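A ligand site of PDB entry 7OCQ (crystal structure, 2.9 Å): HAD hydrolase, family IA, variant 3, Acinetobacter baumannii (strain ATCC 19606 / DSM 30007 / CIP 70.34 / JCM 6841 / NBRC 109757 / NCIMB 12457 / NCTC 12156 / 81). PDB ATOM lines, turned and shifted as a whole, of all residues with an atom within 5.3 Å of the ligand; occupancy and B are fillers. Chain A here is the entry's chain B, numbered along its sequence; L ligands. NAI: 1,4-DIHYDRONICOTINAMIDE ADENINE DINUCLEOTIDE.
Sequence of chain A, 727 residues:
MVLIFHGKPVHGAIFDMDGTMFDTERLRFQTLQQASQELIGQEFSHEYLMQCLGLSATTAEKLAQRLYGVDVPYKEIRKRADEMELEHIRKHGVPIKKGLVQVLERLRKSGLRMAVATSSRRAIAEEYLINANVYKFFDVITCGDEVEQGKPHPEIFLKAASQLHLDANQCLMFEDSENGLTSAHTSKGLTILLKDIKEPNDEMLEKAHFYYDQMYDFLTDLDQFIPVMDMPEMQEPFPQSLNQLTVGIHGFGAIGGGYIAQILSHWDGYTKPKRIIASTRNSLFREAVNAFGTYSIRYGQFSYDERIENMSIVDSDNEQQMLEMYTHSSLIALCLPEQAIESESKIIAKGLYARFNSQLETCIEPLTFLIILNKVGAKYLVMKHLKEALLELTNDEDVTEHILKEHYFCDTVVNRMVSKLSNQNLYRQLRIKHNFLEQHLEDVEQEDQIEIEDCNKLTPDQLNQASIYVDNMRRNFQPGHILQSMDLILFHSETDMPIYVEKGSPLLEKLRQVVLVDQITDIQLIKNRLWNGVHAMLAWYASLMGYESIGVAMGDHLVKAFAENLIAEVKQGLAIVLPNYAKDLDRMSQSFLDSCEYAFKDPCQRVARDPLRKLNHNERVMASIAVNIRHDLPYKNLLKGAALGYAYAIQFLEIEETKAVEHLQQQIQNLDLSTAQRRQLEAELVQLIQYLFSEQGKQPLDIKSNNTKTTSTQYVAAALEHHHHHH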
ATOM      1  N   GLY A 251       7.694 -33.656  -6.261  1.00  0.00           N
ATOM      2  CA  GLY A 251       7.480 -32.493  -5.381  1.00  0.00           C
ATOM      3  C   GLY A 251       7.360 -32.912  -3.930  1.00  0.00           C
ATOM      4  O   GLY A 251       6.222 -33.051  -3.434  1.00  0.00           O
ATOM      5  N   PHE A 252       8.507 -33.097  -3.262  1.00  0.00           N
ATOM      6  CA  PHE A 252       8.597 -33.397  -1.799  1.00  0.00           C
ATOM      7  C   PHE A 252       8.318 -32.111  -1.019  1.00  0.00           C
ATOM      8  O   PHE A 252       9.283 -31.477  -0.520  1.00  0.00           O
ATOM      9  CB  PHE A 252       9.955 -34.009  -1.468  1.00  0.00           C
ATOM     10  CG  PHE A 252      10.113 -34.450  -0.033  1.00  0.00           C
ATOM     11  CD1 PHE A 252       9.392 -35.525   0.456  1.00  0.00           C
ATOM     12  CD2 PHE A 252      10.998 -33.795   0.817  1.00  0.00           C
ATOM     13  CE1 PHE A 252       9.543 -35.926   1.777  1.00  0.00           C
ATOM     14  CE2 PHE A 252      11.139 -34.203   2.131  1.00  0.00           C
ATOM     15  CZ  PHE A 252      10.408 -35.273   2.612  1.00  0.00           C
ATOM     16  N   GLY A 253       7.044 -31.733  -0.938  1.00  0.00           N
ATOM     17  CA  GLY A 253       6.560 -30.526  -0.246  1.00  0.00           C
ATOM     18  C   GLY A 253       5.480 -30.869   0.764  1.00  0.00           C
ATOM     19  O   GLY A 253       5.399 -32.057   1.156  1.00  0.00           O
ATOM     20  N   ALA A 254       4.674 -29.884   1.157  1.00  0.00           N
ATOM     21  CA  ALA A 254       3.575 -30.023   2.145  1.00  0.00           C
ATOM     22  C   ALA A 254       2.742 -31.271   1.835  1.00  0.00           C
ATOM     23  O   ALA A 254       2.672 -32.163   2.697  1.00  0.00           O
ATOM     24  CB  ALA A 254       2.722 -28.772   2.155  1.00  0.00           C
ATOM     25  N   ILE A 255       2.150 -31.332   0.640  1.00  0.00           N
ATOM     26  CA  ILE A 255       1.229 -32.429   0.206  1.00  0.00           C
ATOM     27  C   ILE A 255       2.036 -33.708  -0.019  1.00  0.00           C
ATOM     28  O   ILE A 255       1.706 -34.726   0.626  1.00  0.00           O
ATOM     29  CB  ILE A 255       0.416 -32.009  -1.029  1.00  0.00           C
ATOM     30  CG1 ILE A 255      -0.767 -31.119  -0.659  1.00  0.00           C
ATOM     31  CG2 ILE A 255      -0.037 -33.224  -1.840  1.00  0.00           C
ATOM     32  CD1 ILE A 255      -1.739 -31.736   0.326  1.00  0.00           C
ATOM     33  N   GLY A 256       3.031 -33.668  -0.918  1.00  0.00           N
ATOM     34  CA  GLY A 256       3.839 -34.838  -1.316  1.00  0.00           C
ATOM     35  C   GLY A 256       4.403 -35.570  -0.116  1.00  0.00           C
ATOM     36  O   GLY A 256       4.118 -36.763   0.037  1.00  0.00           O
ATOM     37  N   SER A 279      11.178 -35.991  -5.292  1.00  0.00           N
ATOM     38  CA  SER A 279      12.016 -34.923  -5.902  1.00  0.00           C
ATOM     39  C   SER A 279      11.709 -33.577  -5.230  1.00  0.00           C
ATOM     40  O   SER A 279      10.524 -33.272  -5.039  1.00  0.00           O
ATOM     41  CB  SER A 279      11.804 -34.853  -7.392  1.00  0.00           C
ATOM     42  OG  SER A 279      10.554 -34.238  -7.705  1.00  0.00           O
ATOM     43  N   THR A 280      12.752 -32.804  -4.898  1.00  0.00           N
ATOM     44  CA  THR A 280      12.664 -31.446  -4.306  1.00  0.00           C
ATOM     45  C   THR A 280      13.867 -30.597  -4.743  1.00  0.00           C
ATOM     46  O   THR A 280      14.950 -31.181  -4.965  1.00  0.00           O
ATOM     47  CB  THR A 280      12.571 -31.502  -2.772  1.00  0.00           C
ATOM     48  OG1 THR A 280      12.436 -30.163  -2.281  1.00  0.00           O
ATOM     49  CG2 THR A 280      13.766 -32.167  -2.124  1.00  0.00           C
ATOM     50  N   ARG A 281      13.669 -29.282  -4.840  1.00  0.00           N
ATOM     51  CA  ARG A 281      14.735 -28.275  -5.091  1.00  0.00           C
ATOM     52  C   ARG A 281      15.338 -27.842  -3.744  1.00  0.00           C
ATOM     53  O   ARG A 281      16.496 -27.379  -3.743  1.00  0.00           O
ATOM     54  CB  ARG A 281      14.178 -27.093  -5.877  1.00  0.00           C
ATOM     55  CG  ARG A 281      13.442 -27.507  -7.150  1.00  0.00           C
ATOM     56  CD  ARG A 281      13.652 -26.547  -8.312  1.00  0.00           C
ATOM     57  NE  ARG A 281      13.335 -27.176  -9.587  1.00  0.00           N
ATOM     58  CZ  ARG A 281      13.447 -26.595 -10.777  1.00  0.00           C
ATOM     59  NH1 ARG A 281      13.137 -27.268 -11.873  1.00  0.00           N
ATOM     60  NH2 ARG A 281      13.868 -25.340 -10.871  1.00  0.00           N
ATOM     61  N   ASN A 282      14.571 -27.984  -2.652  1.00  0.00           N
ATOM     62  CA  ASN A 282      15.013 -27.681  -1.260  1.00  0.00           C
ATOM     63  C   ASN A 282      16.103 -28.681  -0.861  1.00  0.00           C
ATOM     64  O   ASN A 282      15.761 -29.821  -0.491  1.00  0.00           O
ATOM     65  CB  ASN A 282      13.824 -27.689  -0.290  1.00  0.00           C
ATOM     66  CG  ASN A 282      14.114 -26.982   1.022  1.00  0.00           C
ATOM     67  OD1 ASN A 282      15.219 -27.066   1.543  1.00  0.00           O
ATOM     68  ND2 ASN A 282      13.121 -26.295   1.559  1.00  0.00           N
ATOM     69  N   SER A 316      15.481 -32.307  -8.302  1.00  0.00           N
ATOM     70  CA  SER A 316      14.538 -32.114  -9.445  1.00  0.00           C
ATOM     71  C   SER A 316      15.327 -31.835 -10.738  1.00  0.00           C
ATOM     72  O   SER A 316      14.801 -32.182 -11.818  1.00  0.00           O
ATOM     73  CB  SER A 316      13.554 -31.016  -9.157  1.00  0.00           C
ATOM     74  OG  SER A 316      12.661 -31.381  -8.122  1.00  0.00           O
ATOM     75  N   CYS A 335       2.928 -33.309  -7.223  1.00  0.00           N
ATOM     76  CA  CYS A 335       2.623 -32.396  -6.085  1.00  0.00           C
ATOM     77  C   CYS A 335       3.372 -31.072  -6.287  1.00  0.00           C
ATOM     78  O   CYS A 335       4.160 -30.688  -5.386  1.00  0.00           O
ATOM     79  CB  CYS A 335       3.010 -33.052  -4.758  1.00  0.00           C
ATOM     80  SG  CYS A 335       2.372 -34.735  -4.579  1.00  0.00           S
ATOM     81  N   LEU A 336       3.136 -30.407  -7.421  1.00  0.00           N
ATOM     82  CA  LEU A 336       3.781 -29.119  -7.809  1.00  0.00           C
ATOM     83  C   LEU A 336       2.707 -28.033  -7.943  1.00  0.00           C
ATOM     84  O   LEU A 336       1.597 -28.323  -8.386  1.00  0.00           O
ATOM     85  CB  LEU A 336       4.535 -29.301  -9.127  1.00  0.00           C
ATOM     86  CG  LEU A 336       5.738 -30.230  -9.092  1.00  0.00           C
ATOM     87  CD1 LEU A 336       6.265 -30.471 -10.493  1.00  0.00           C
ATOM     88  CD2 LEU A 336       6.837 -29.675  -8.203  1.00  0.00           C
ATOM     89  N   PRO A 337       3.015 -26.763  -7.581  1.00  0.00           N
ATOM     90  CA  PRO A 337       2.135 -25.635  -7.894  1.00  0.00           C
ATOM     91  C   PRO A 337       2.028 -25.379  -9.413  1.00  0.00           C
ATOM     92  O   PRO A 337       2.850 -25.892 -10.143  1.00  0.00           O
ATOM     93  CB  PRO A 337       2.805 -24.424  -7.216  1.00  0.00           C
ATOM     94  CG  PRO A 337       3.764 -25.024  -6.210  1.00  0.00           C
ATOM     95  CD  PRO A 337       4.199 -26.350  -6.809  1.00  0.00           C
ATOM     96  N   GLU A 338       1.036 -24.582  -9.816  1.00  0.00           N
ATOM     97  CA  GLU A 338       0.750 -24.230 -11.239  1.00  0.00           C
ATOM     98  C   GLU A 338       1.985 -23.604 -11.888  1.00  0.00           C
ATOM     99  O   GLU A 338       2.210 -23.855 -13.097  1.00  0.00           O
ATOM    100  CB  GLU A 338      -0.429 -23.260 -11.335  1.00  0.00           C
ATOM    101  CG  GLU A 338      -1.780 -23.898 -11.048  1.00  0.00           C
ATOM    102  CD  GLU A 338      -2.977 -23.094 -11.532  1.00  0.00           C
ATOM    103  OE1 GLU A 338      -3.853 -22.778 -10.705  1.00  0.00           O
ATOM    104  OE2 GLU A 338      -3.024 -22.794 -12.746  1.00  0.00           O
ATOM    105  N   GLN A 339       2.752 -22.813 -11.121  1.00  0.00           N
ATOM    106  CA  GLN A 339       3.921 -22.029 -11.597  1.00  0.00           C
ATOM    107  C   GLN A 339       4.989 -22.971 -12.191  1.00  0.00           C
ATOM    108  O   GLN A 339       5.678 -22.545 -13.141  1.00  0.00           O
ATOM    109  CB  GLN A 339       4.516 -21.199 -10.461  1.00  0.00           C
ATOM    110  CG  GLN A 339       3.563 -20.149  -9.897  1.00  0.00           C
ATOM    111  CD  GLN A 339       2.755 -20.643  -8.717  1.00  0.00           C
ATOM    112  OE1 GLN A 339       1.522 -20.642  -8.741  1.00  0.00           O
ATOM    113  NE2 GLN A 339       3.441 -21.065  -7.672  1.00  0.00           N
ATOM    114  N   ALA A 340       5.120 -24.177 -11.645  1.00  0.00           N
ATOM    115  CA  ALA A 340       6.197 -25.146 -11.957  1.00  0.00           C
ATOM    116  C   ALA A 340       5.759 -26.155 -13.033  1.00  0.00           C
ATOM    117  O   ALA A 340       6.648 -26.825 -13.589  1.00  0.00           O
ATOM    118  CB  ALA A 340       6.602 -25.867 -10.696  1.00  0.00           C
ATOM    119  N   SER A 343       7.554 -25.761 -16.669  1.00  0.00           N
ATOM    120  CA  SER A 343       9.018 -26.024 -16.637  1.00  0.00           C
ATOM    121  C   SER A 343       9.280 -27.518 -16.396  1.00  0.00           C
ATOM    122  O   SER A 343      10.188 -28.069 -17.047  1.00  0.00           O
ATOM    123  CB  SER A 343       9.705 -25.172 -15.604  1.00  0.00           C
ATOM    124  OG  SER A 343       9.280 -25.525 -14.289  1.00  0.00           O
ATOM    125  N   GLU A 344       8.502 -28.146 -15.505  1.00  0.00           N
ATOM    126  CA  GLU A 344       8.718 -29.550 -15.032  1.00  0.00           C
ATOM    127  C   GLU A 344       8.120 -30.554 -16.025  1.00  0.00           C
ATOM    128  O   GLU A 344       8.543 -31.731 -15.983  1.00  0.00           O
ATOM    129  CB  GLU A 344       8.139 -29.750 -13.631  1.00  0.00           C
ATOM    130  CG  GLU A 344       9.057 -29.236 -12.525  1.00  0.00           C
ATOM    131  CD  GLU A 344      10.227 -30.137 -12.197  1.00  0.00           C
ATOM    132  OE1 GLU A 344      10.872 -29.909 -11.150  1.00  0.00           O
ATOM    133  OE2 GLU A 344      10.516 -31.069 -12.972  1.00  0.00           O
ATOM    134  N   ILE A 372      -2.038 -33.908  -8.194  1.00  0.00           N
ATOM    135  CA  ILE A 372      -2.475 -33.132  -6.988  1.00  0.00           C
ATOM    136  C   ILE A 372      -2.254 -31.648  -7.277  1.00  0.00           C
ATOM    137  O   ILE A 372      -1.082 -31.229  -7.374  1.00  0.00           O
ATOM    138  CB  ILE A 372      -1.728 -33.574  -5.709  1.00  0.00           C
ATOM    139  CG1 ILE A 372      -1.410 -35.079  -5.686  1.00  0.00           C
ATOM    140  CG2 ILE A 372      -2.516 -33.154  -4.483  1.00  0.00           C
ATOM    141  CD1 ILE A 372      -2.629 -35.969  -5.674  1.00  0.00           C
ATOM    142  N   LEU A 373      -3.345 -30.889  -7.437  1.00  0.00           N
ATOM    143  CA  LEU A 373      -3.321 -29.455  -7.830  1.00  0.00           C
ATOM    144  C   LEU A 373      -4.707 -28.835  -7.575  1.00  0.00           C
ATOM    145  O   LEU A 373      -5.691 -29.378  -8.102  1.00  0.00           O
ATOM    146  CB  LEU A 373      -2.912 -29.347  -9.300  1.00  0.00           C
ATOM    147  CG  LEU A 373      -2.791 -27.936  -9.881  1.00  0.00           C
ATOM    148  CD1 LEU A 373      -1.692 -27.152  -9.188  1.00  0.00           C
ATOM    149  CD2 LEU A 373      -2.537 -27.989 -11.379  1.00  0.00           C
ATOM    150  N   ASN A 374      -4.763 -27.762  -6.784  1.00  0.00           N
ATOM    151  CA  ASN A 374      -6.010 -26.997  -6.505  1.00  0.00           C
ATOM    152  C   ASN A 374      -6.258 -26.021  -7.657  1.00  0.00           C
ATOM    153  O   ASN A 374      -5.758 -24.874  -7.605  1.00  0.00           O
ATOM    154  CB  ASN A 374      -5.953 -26.260  -5.151  1.00  0.00           C
ATOM    155  CG  ASN A 374      -6.125 -27.175  -3.961  1.00  0.00           C
ATOM    156  OD1 ASN A 374      -6.424 -28.355  -4.108  1.00  0.00           O
ATOM    157  ND2 ASN A 374      -5.960 -26.631  -2.772  1.00  0.00           N
ATOM    158  N   VAL A 414      -7.967 -33.275  -2.824  1.00  0.00           N
ATOM    159  CA  VAL A 414      -7.248 -33.363  -1.517  1.00  0.00           C
ATOM    160  C   VAL A 414      -7.813 -32.293  -0.575  1.00  0.00           C
ATOM    161  O   VAL A 414      -7.608 -31.099  -0.860  1.00  0.00           O
ATOM    162  CB  VAL A 414      -5.723 -33.199  -1.708  1.00  0.00           C
ATOM    163  CG1 VAL A 414      -4.996 -32.997  -0.383  1.00  0.00           C
ATOM    164  CG2 VAL A 414      -5.135 -34.370  -2.466  1.00  0.00           C
ATOM    165  N   ARG A 416      -7.119 -32.335   2.851  1.00  0.00           N
ATOM    166  CA  ARG A 416      -6.191 -32.245   4.010  1.00  0.00           C
ATOM    167  C   ARG A 416      -5.374 -30.944   3.924  1.00  0.00           C
ATOM    168  O   ARG A 416      -4.851 -30.646   2.842  1.00  0.00           O
ATOM    169  CB  ARG A 416      -5.244 -33.449   4.063  1.00  0.00           C
ATOM    170  CG  ARG A 416      -4.255 -33.399   5.225  1.00  0.00           C
ATOM    171  CD  ARG A 416      -3.255 -34.532   5.217  1.00  0.00           C
ATOM    172  NE  ARG A 416      -3.761 -35.732   5.883  1.00  0.00           N
ATOM    173  CZ  ARG A 416      -3.015 -36.741   6.319  1.00  0.00           C
ATOM    174  NH1 ARG A 416      -1.703 -36.730   6.171  1.00  0.00           N
ATOM    175  NH2 ARG A 416      -3.590 -37.774   6.917  1.00  0.00           N
ATOM    176  N   MET A 417      -5.283 -30.226   5.058  1.00  0.00           N
ATOM    177  CA  MET A 417      -4.438 -29.017   5.239  1.00  0.00           C
ATOM    178  C   MET A 417      -3.085 -29.453   5.839  1.00  0.00           C
ATOM    179  O   MET A 417      -3.085 -29.925   6.990  1.00  0.00           O
ATOM    180  CB  MET A 417      -5.110 -28.027   6.187  1.00  0.00           C
ATOM    181  CG  MET A 417      -6.484 -27.581   5.730  1.00  0.00           C
ATOM    182  SD  MET A 417      -7.329 -26.554   6.954  1.00  0.00           S
ATOM    183  CE  MET A 417      -8.884 -26.264   6.109  1.00  0.00           C
ATOM    184  N   VAL A 418      -2.000 -29.301   5.065  1.00  0.00           N
ATOM    185  CA  VAL A 418      -0.611 -29.663   5.483  1.00  0.00           C
ATOM    186  C   VAL A 418       0.275 -28.411   5.355  1.00  0.00           C
ATOM    187  O   VAL A 418       0.007 -27.577   4.477  1.00  0.00           O
ATOM    188  CB  VAL A 418      -0.051 -30.829   4.660  1.00  0.00           C
ATOM    189  CG1 VAL A 418       1.188 -31.422   5.312  1.00  0.00           C
ATOM    190  CG2 VAL A 418      -1.091 -31.918   4.432  1.00  0.00           C
ATOM    191  N   LYS A 420       4.482 -27.086   5.325  1.00  0.00           N
ATOM    192  CA  LYS A 420       5.940 -27.326   5.202  1.00  0.00           C
ATOM    193  C   LYS A 420       6.667 -26.527   6.307  1.00  0.00           C
ATOM    194  O   LYS A 420       6.254 -25.386   6.569  1.00  0.00           O
ATOM    195  CB  LYS A 420       6.429 -26.902   3.812  1.00  0.00           C
ATOM    196  CG  LYS A 420       7.803 -27.434   3.410  1.00  0.00           C
ATOM    197  CD  LYS A 420       8.234 -26.997   2.027  1.00  0.00           C
ATOM    198  CE  LYS A 420       9.453 -27.741   1.525  1.00  0.00           C
ATOM    199  NZ  LYS A 420       9.993 -27.149   0.280  1.00  0.00           N
ATOM    200  N   LYS A 527     -15.113 -27.641  -4.265  1.00  0.00           N
ATOM    201  CA  LYS A 527     -13.814 -27.636  -3.527  1.00  0.00           C
ATOM    202  C   LYS A 527     -13.122 -26.279  -3.743  1.00  0.00           C
ATOM    203  O   LYS A 527     -12.714 -25.669  -2.739  1.00  0.00           O
ATOM    204  CB  LYS A 527     -12.950 -28.814  -4.005  1.00  0.00           C
ATOM    205  CG  LYS A 527     -11.467 -28.743  -3.664  1.00  0.00           C
ATOM    206  CD  LYS A 527     -11.156 -28.839  -2.195  1.00  0.00           C
ATOM    207  CE  LYS A 527      -9.664 -28.911  -1.925  1.00  0.00           C
ATOM    208  NZ  LYS A 527      -9.354 -28.682  -0.488  1.00  0.00           N
ATOM    209  N   ASN A 532     -11.375 -23.801  -0.868  1.00  0.00           N
ATOM    210  CA  ASN A 532     -10.096 -23.094  -1.146  1.00  0.00           C
ATOM    211  C   ASN A 532     -10.336 -21.574  -1.247  1.00  0.00           C
ATOM    212  O   ASN A 532      -9.399 -20.819  -0.922  1.00  0.00           O
ATOM    213  CB  ASN A 532      -9.428 -23.604  -2.425  1.00  0.00           C
ATOM    214  CG  ASN A 532      -9.085 -25.079  -2.369  1.00  0.00           C
ATOM    215  OD1 ASN A 532      -9.374 -25.818  -3.312  1.00  0.00           O
ATOM    216  ND2 ASN A 532      -8.487 -25.515  -1.274  1.00  0.00           N
ATOM    217  N   ARG A 606       1.005 -19.571   3.808  1.00  0.00           N
ATOM    218  CA  ARG A 606       0.848 -20.731   2.879  1.00  0.00           C
ATOM    219  C   ARG A 606      -0.505 -20.652   2.165  1.00  0.00           C
ATOM    220  O   ARG A 606      -0.559 -20.967   0.964  1.00  0.00           O
ATOM    221  CB  ARG A 606       0.975 -22.038   3.661  1.00  0.00           C
ATOM    222  CG  ARG A 606       1.032 -23.290   2.792  1.00  0.00           C
ATOM    223  CD  ARG A 606       0.778 -24.550   3.590  1.00  0.00           C
ATOM    224  NE  ARG A 606      -0.590 -24.595   4.115  1.00  0.00           N
ATOM    225  CZ  ARG A 606      -1.669 -24.926   3.421  1.00  0.00           C
ATOM    226  NH1 ARG A 606      -1.580 -25.246   2.132  1.00  0.00           N
ATOM    227  NH2 ARG A 606      -2.856 -24.936   4.002  1.00  0.00           N
ATOM    228  N   ARG A 609      -0.716 -17.662  -0.507  1.00  0.00           N
ATOM    229  CA  ARG A 609       0.242 -17.722  -1.643  1.00  0.00           C
ATOM    230  C   ARG A 609      -0.454 -17.193  -2.898  1.00  0.00           C
ATOM    231  O   ARG A 609      -1.696 -17.328  -2.978  1.00  0.00           O
ATOM    232  CB  ARG A 609       0.714 -19.160  -1.924  1.00  0.00           C
ATOM    233  CG  ARG A 609       1.952 -19.587  -1.150  1.00  0.00           C
ATOM    234  CD  ARG A 609       2.355 -21.028  -1.461  1.00  0.00           C
ATOM    235  NE  ARG A 609       1.217 -21.930  -1.517  1.00  0.00           N
ATOM    236  CZ  ARG A 609       1.229 -23.239  -1.234  1.00  0.00           C
ATOM    237  NH1 ARG A 609       0.114 -23.937  -1.325  1.00  0.00           N
ATOM    238  NH2 ARG A 609       2.346 -23.835  -0.847  1.00  0.00           N
HETATM  239  PA  NAI L   1       4.960 -26.372  -1.557  1.00  0.00           P
HETATM  240  O1A NAI L   1       5.346 -25.046  -2.125  1.00  0.00           O
HETATM  241  O2A NAI L   1       5.256 -26.631  -0.119  1.00  0.00           O
HETATM  242  O5B NAI L   1       5.602 -27.538  -2.448  1.00  0.00           O
HETATM  243  C5B NAI L   1       7.041 -27.645  -2.391  1.00  0.00           C
HETATM  244  C4B NAI L   1       7.528 -28.745  -3.298  1.00  0.00           C
HETATM  245  O4B NAI L   1       7.359 -28.332  -4.676  1.00  0.00           O
HETATM  246  C3B NAI L   1       9.012 -29.104  -3.163  1.00  0.00           C
HETATM  247  O3B NAI L   1       9.266 -30.457  -3.492  1.00  0.00           O
HETATM  248  C2B NAI L   1       9.641 -28.143  -4.175  1.00  0.00           C
HETATM  249  O2B NAI L   1      10.923 -28.558  -4.604  1.00  0.00           O
HETATM  250  C1B NAI L   1       8.615 -28.214  -5.293  1.00  0.00           C
HETATM  251  N9A NAI L   1       8.613 -27.033  -6.153  1.00  0.00           N
HETATM  252  C8A NAI L   1       8.056 -25.810  -5.869  1.00  0.00           C
HETATM  253  N7A NAI L   1       8.213 -24.932  -6.832  1.00  0.00           N
HETATM  254  C5A NAI L   1       8.930 -25.609  -7.806  1.00  0.00           C
HETATM  255  C6A NAI L   1       9.423 -25.218  -9.071  1.00  0.00           C
HETATM  256  N6A NAI L   1       9.250 -24.004  -9.582  1.00  0.00           N
HETATM  257  N1A NAI L   1      10.093 -26.145  -9.790  1.00  0.00           N
HETATM  258  C2A NAI L   1      10.262 -27.365  -9.266  1.00  0.00           C
HETATM  259  N3A NAI L   1       9.855 -27.849  -8.089  1.00  0.00           N
HETATM  260  C4A NAI L   1       9.192 -26.908  -7.394  1.00  0.00           C
HETATM  261  O3  NAI L   1       3.381 -26.584  -1.789  1.00  0.00           O
HETATM  262  PN  NAI L   1       2.427 -27.870  -1.827  1.00  0.00           P
HETATM  263  O1N NAI L   1       1.273 -27.624  -0.919  1.00  0.00           O
HETATM  264  O2N NAI L   1       3.253 -29.095  -1.619  1.00  0.00           O
HETATM  265  O5D NAI L   1       1.932 -27.802  -3.341  1.00  0.00           O
HETATM  266  C5D NAI L   1       1.535 -29.006  -4.045  1.00  0.00           C
HETATM  267  C4D NAI L   1       0.117 -28.852  -4.541  1.00  0.00           C
HETATM  268  O4D NAI L   1      -0.794 -29.368  -3.548  1.00  0.00           O
HETATM  269  C3D NAI L   1      -0.351 -27.415  -4.850  1.00  0.00           C
HETATM  270  O3D NAI L   1      -0.559 -27.251  -6.249  1.00  0.00           O
HETATM  271  C2D NAI L   1      -1.646 -27.281  -4.039  1.00  0.00           C
HETATM  272  O2D NAI L   1      -2.679 -26.657  -4.791  1.00  0.00           O
HETATM  273  C1D NAI L   1      -2.026 -28.712  -3.690  1.00  0.00           C
HETATM  274  N1N NAI L   1      -2.793 -28.835  -2.409  1.00  0.00           N
HETATM  275  C2N NAI L   1      -2.307 -28.324  -1.238  1.00  0.00           C
HETATM  276  C3N NAI L   1      -2.995 -28.455  -0.057  1.00  0.00           C
HETATM  277  C7N NAI L   1      -2.259 -28.288   1.225  1.00  0.00           C
HETATM  278  O7N NAI L   1      -2.891 -28.229   2.288  1.00  0.00           O
HETATM  279  N7N NAI L   1      -0.943 -28.196   1.210  1.00  0.00           N
HETATM  280  C4N NAI L   1      -4.458 -28.772  -0.122  1.00  0.00           C
HETATM  281  C5N NAI L   1      -4.884 -29.250  -1.451  1.00  0.00           C
HETATM  282  C6N NAI L   1      -4.009 -29.490  -2.396  1.00  0.00           C
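An oxygen (O2B) of the ligand sits at hydrogen-bond distance from the side-chain hydroxyl of Thr 280 (3.2 Å).
An oxygen (O2B) of the ligand is in hydrogen-bond range of the backbone NH of Arg 281 (2.8 Å).
The backbone NH (N) of Val 418 lies within hydrogen-bond range of an oxygen (O7N) of the ligand (3.1 Å).
An oxygen (O1A) of the ligand is in salt-bridge range of the guanidinium group (NH2) of Arg 609, at 3.5 Å.
The backbone carbonyl oxygen of Leu 336 lies within hydrogen-bond range of an oxygen (O3D) of the ligand, at 3.2 Å.
An oxygen (O2N) of the ligand lies within hydrogen-bond range of the backbone NH (N) of Ile 255 (3.4 Å).
NE of Arg 281 sits close to N1A of the ligand, at 3.4 Å.
N of Asn 374 is in hydrogen-bond range of O2D of the ligand, 3.1 Å away.
O3B of the ligand is in hydrogen-bond range of N of Phe 252 (2.8 Å).
O of Val 418 lies within hydrogen-bond range of N7N of the ligand (3.5 Å).
O3B of the ligand lies close to O of Phe 252, at 3.1 Å.
The backbone carbonyl oxygen (O) of Ser 279 sits at hydrogen-bond distance from an oxygen (O3B) of the ligand (3.4 Å).
O7N of the ligand sits close to NH1 of Arg 606 (3.3 Å).
The backbone NH of Ala 254 is in hydrogen-bond range of an oxygen (O2N) of the ligand (3.2 Å).
The backbone carbonyl oxygen (O) of Arg 416 lies close to an oxygen (O7N) of the ligand (3.2 Å).
Gly 251 touches the ligand (C to O3B, 3.1 Å).
Gly 253 touches the ligand.
Cys 335 touches the ligand (O to C5D, 3.4 Å).
Pro 337 touches the ligand.
Ala 340 touches the ligand (CB to C6A, 3.3 Å).
Glu 344 touches the ligand (OE1 to C2A, 3.2 Å).
Ile 372 touches the ligand.
Leu 373 touches the ligand.
O of Val 414 touches C5N of the ligand, at 3.3 Å.
CA of Met 417 touches O7N of the ligand, 3.4 Å away.
Lys 420 touches the ligand (CD to O2A, 3.7 Å).
Hydrophobic or aromatic side chains within 4 Å of the ligand: Ala 254, Ile 255, Leu 336, Ala 340, Leu 373 and Val 414.
23 residues have an atom within 4 Å of the ligand: Gly 251, Phe 252, Gly 253, Ala 254, Ile 255, Ser 279, Thr 280, Arg 281, Cys 335, Leu 336, Pro 337, Ala 340, Glu 344, Ile 372, Leu 373, Asn 374, Val 414, Arg 416, Met 417, Val 418, Lys 420, Arg 606 and Arg 609.
The nearest printed residue that does not touch the ligand is Asn 282 (4.2 Å).
The side-chain amino group (NZ) of Lys 420 sits close to the side-chain amide nitrogen (ND2) of Asn 282 (3.5 Å).
The backbone carbonyl oxygen (O) of Val 418 lies within hydrogen-bond range of the guanidinium group (NE) of Arg 606 (3.1 Å).
The backbone carbonyl oxygen of Arg 606 sits at hydrogen-bond distance from the guanidinium group of Arg 609, 3.2 Å away.
The guanidinium group (NH1) of Arg 281 lies within salt-bridge range of the side-chain carboxylate (OE1) of Glu 344, 3.6 Å away.
The side-chain amide nitrogen of Asn 374 sits close to the side-chain amide nitrogen of Asn 532 (3.1 Å).
The backbone carbonyl oxygen of Ser 279 is in hydrogen-bond range of the backbone NH of Gly 251.
The backbone NH of Phe 252 is in hydrogen-bond range of the backbone carbonyl oxygen of Ser 279 (2.7 Å).
O of Val 414 sits at hydrogen-bond distance from NZ of Lys 527 (3.0 Å).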
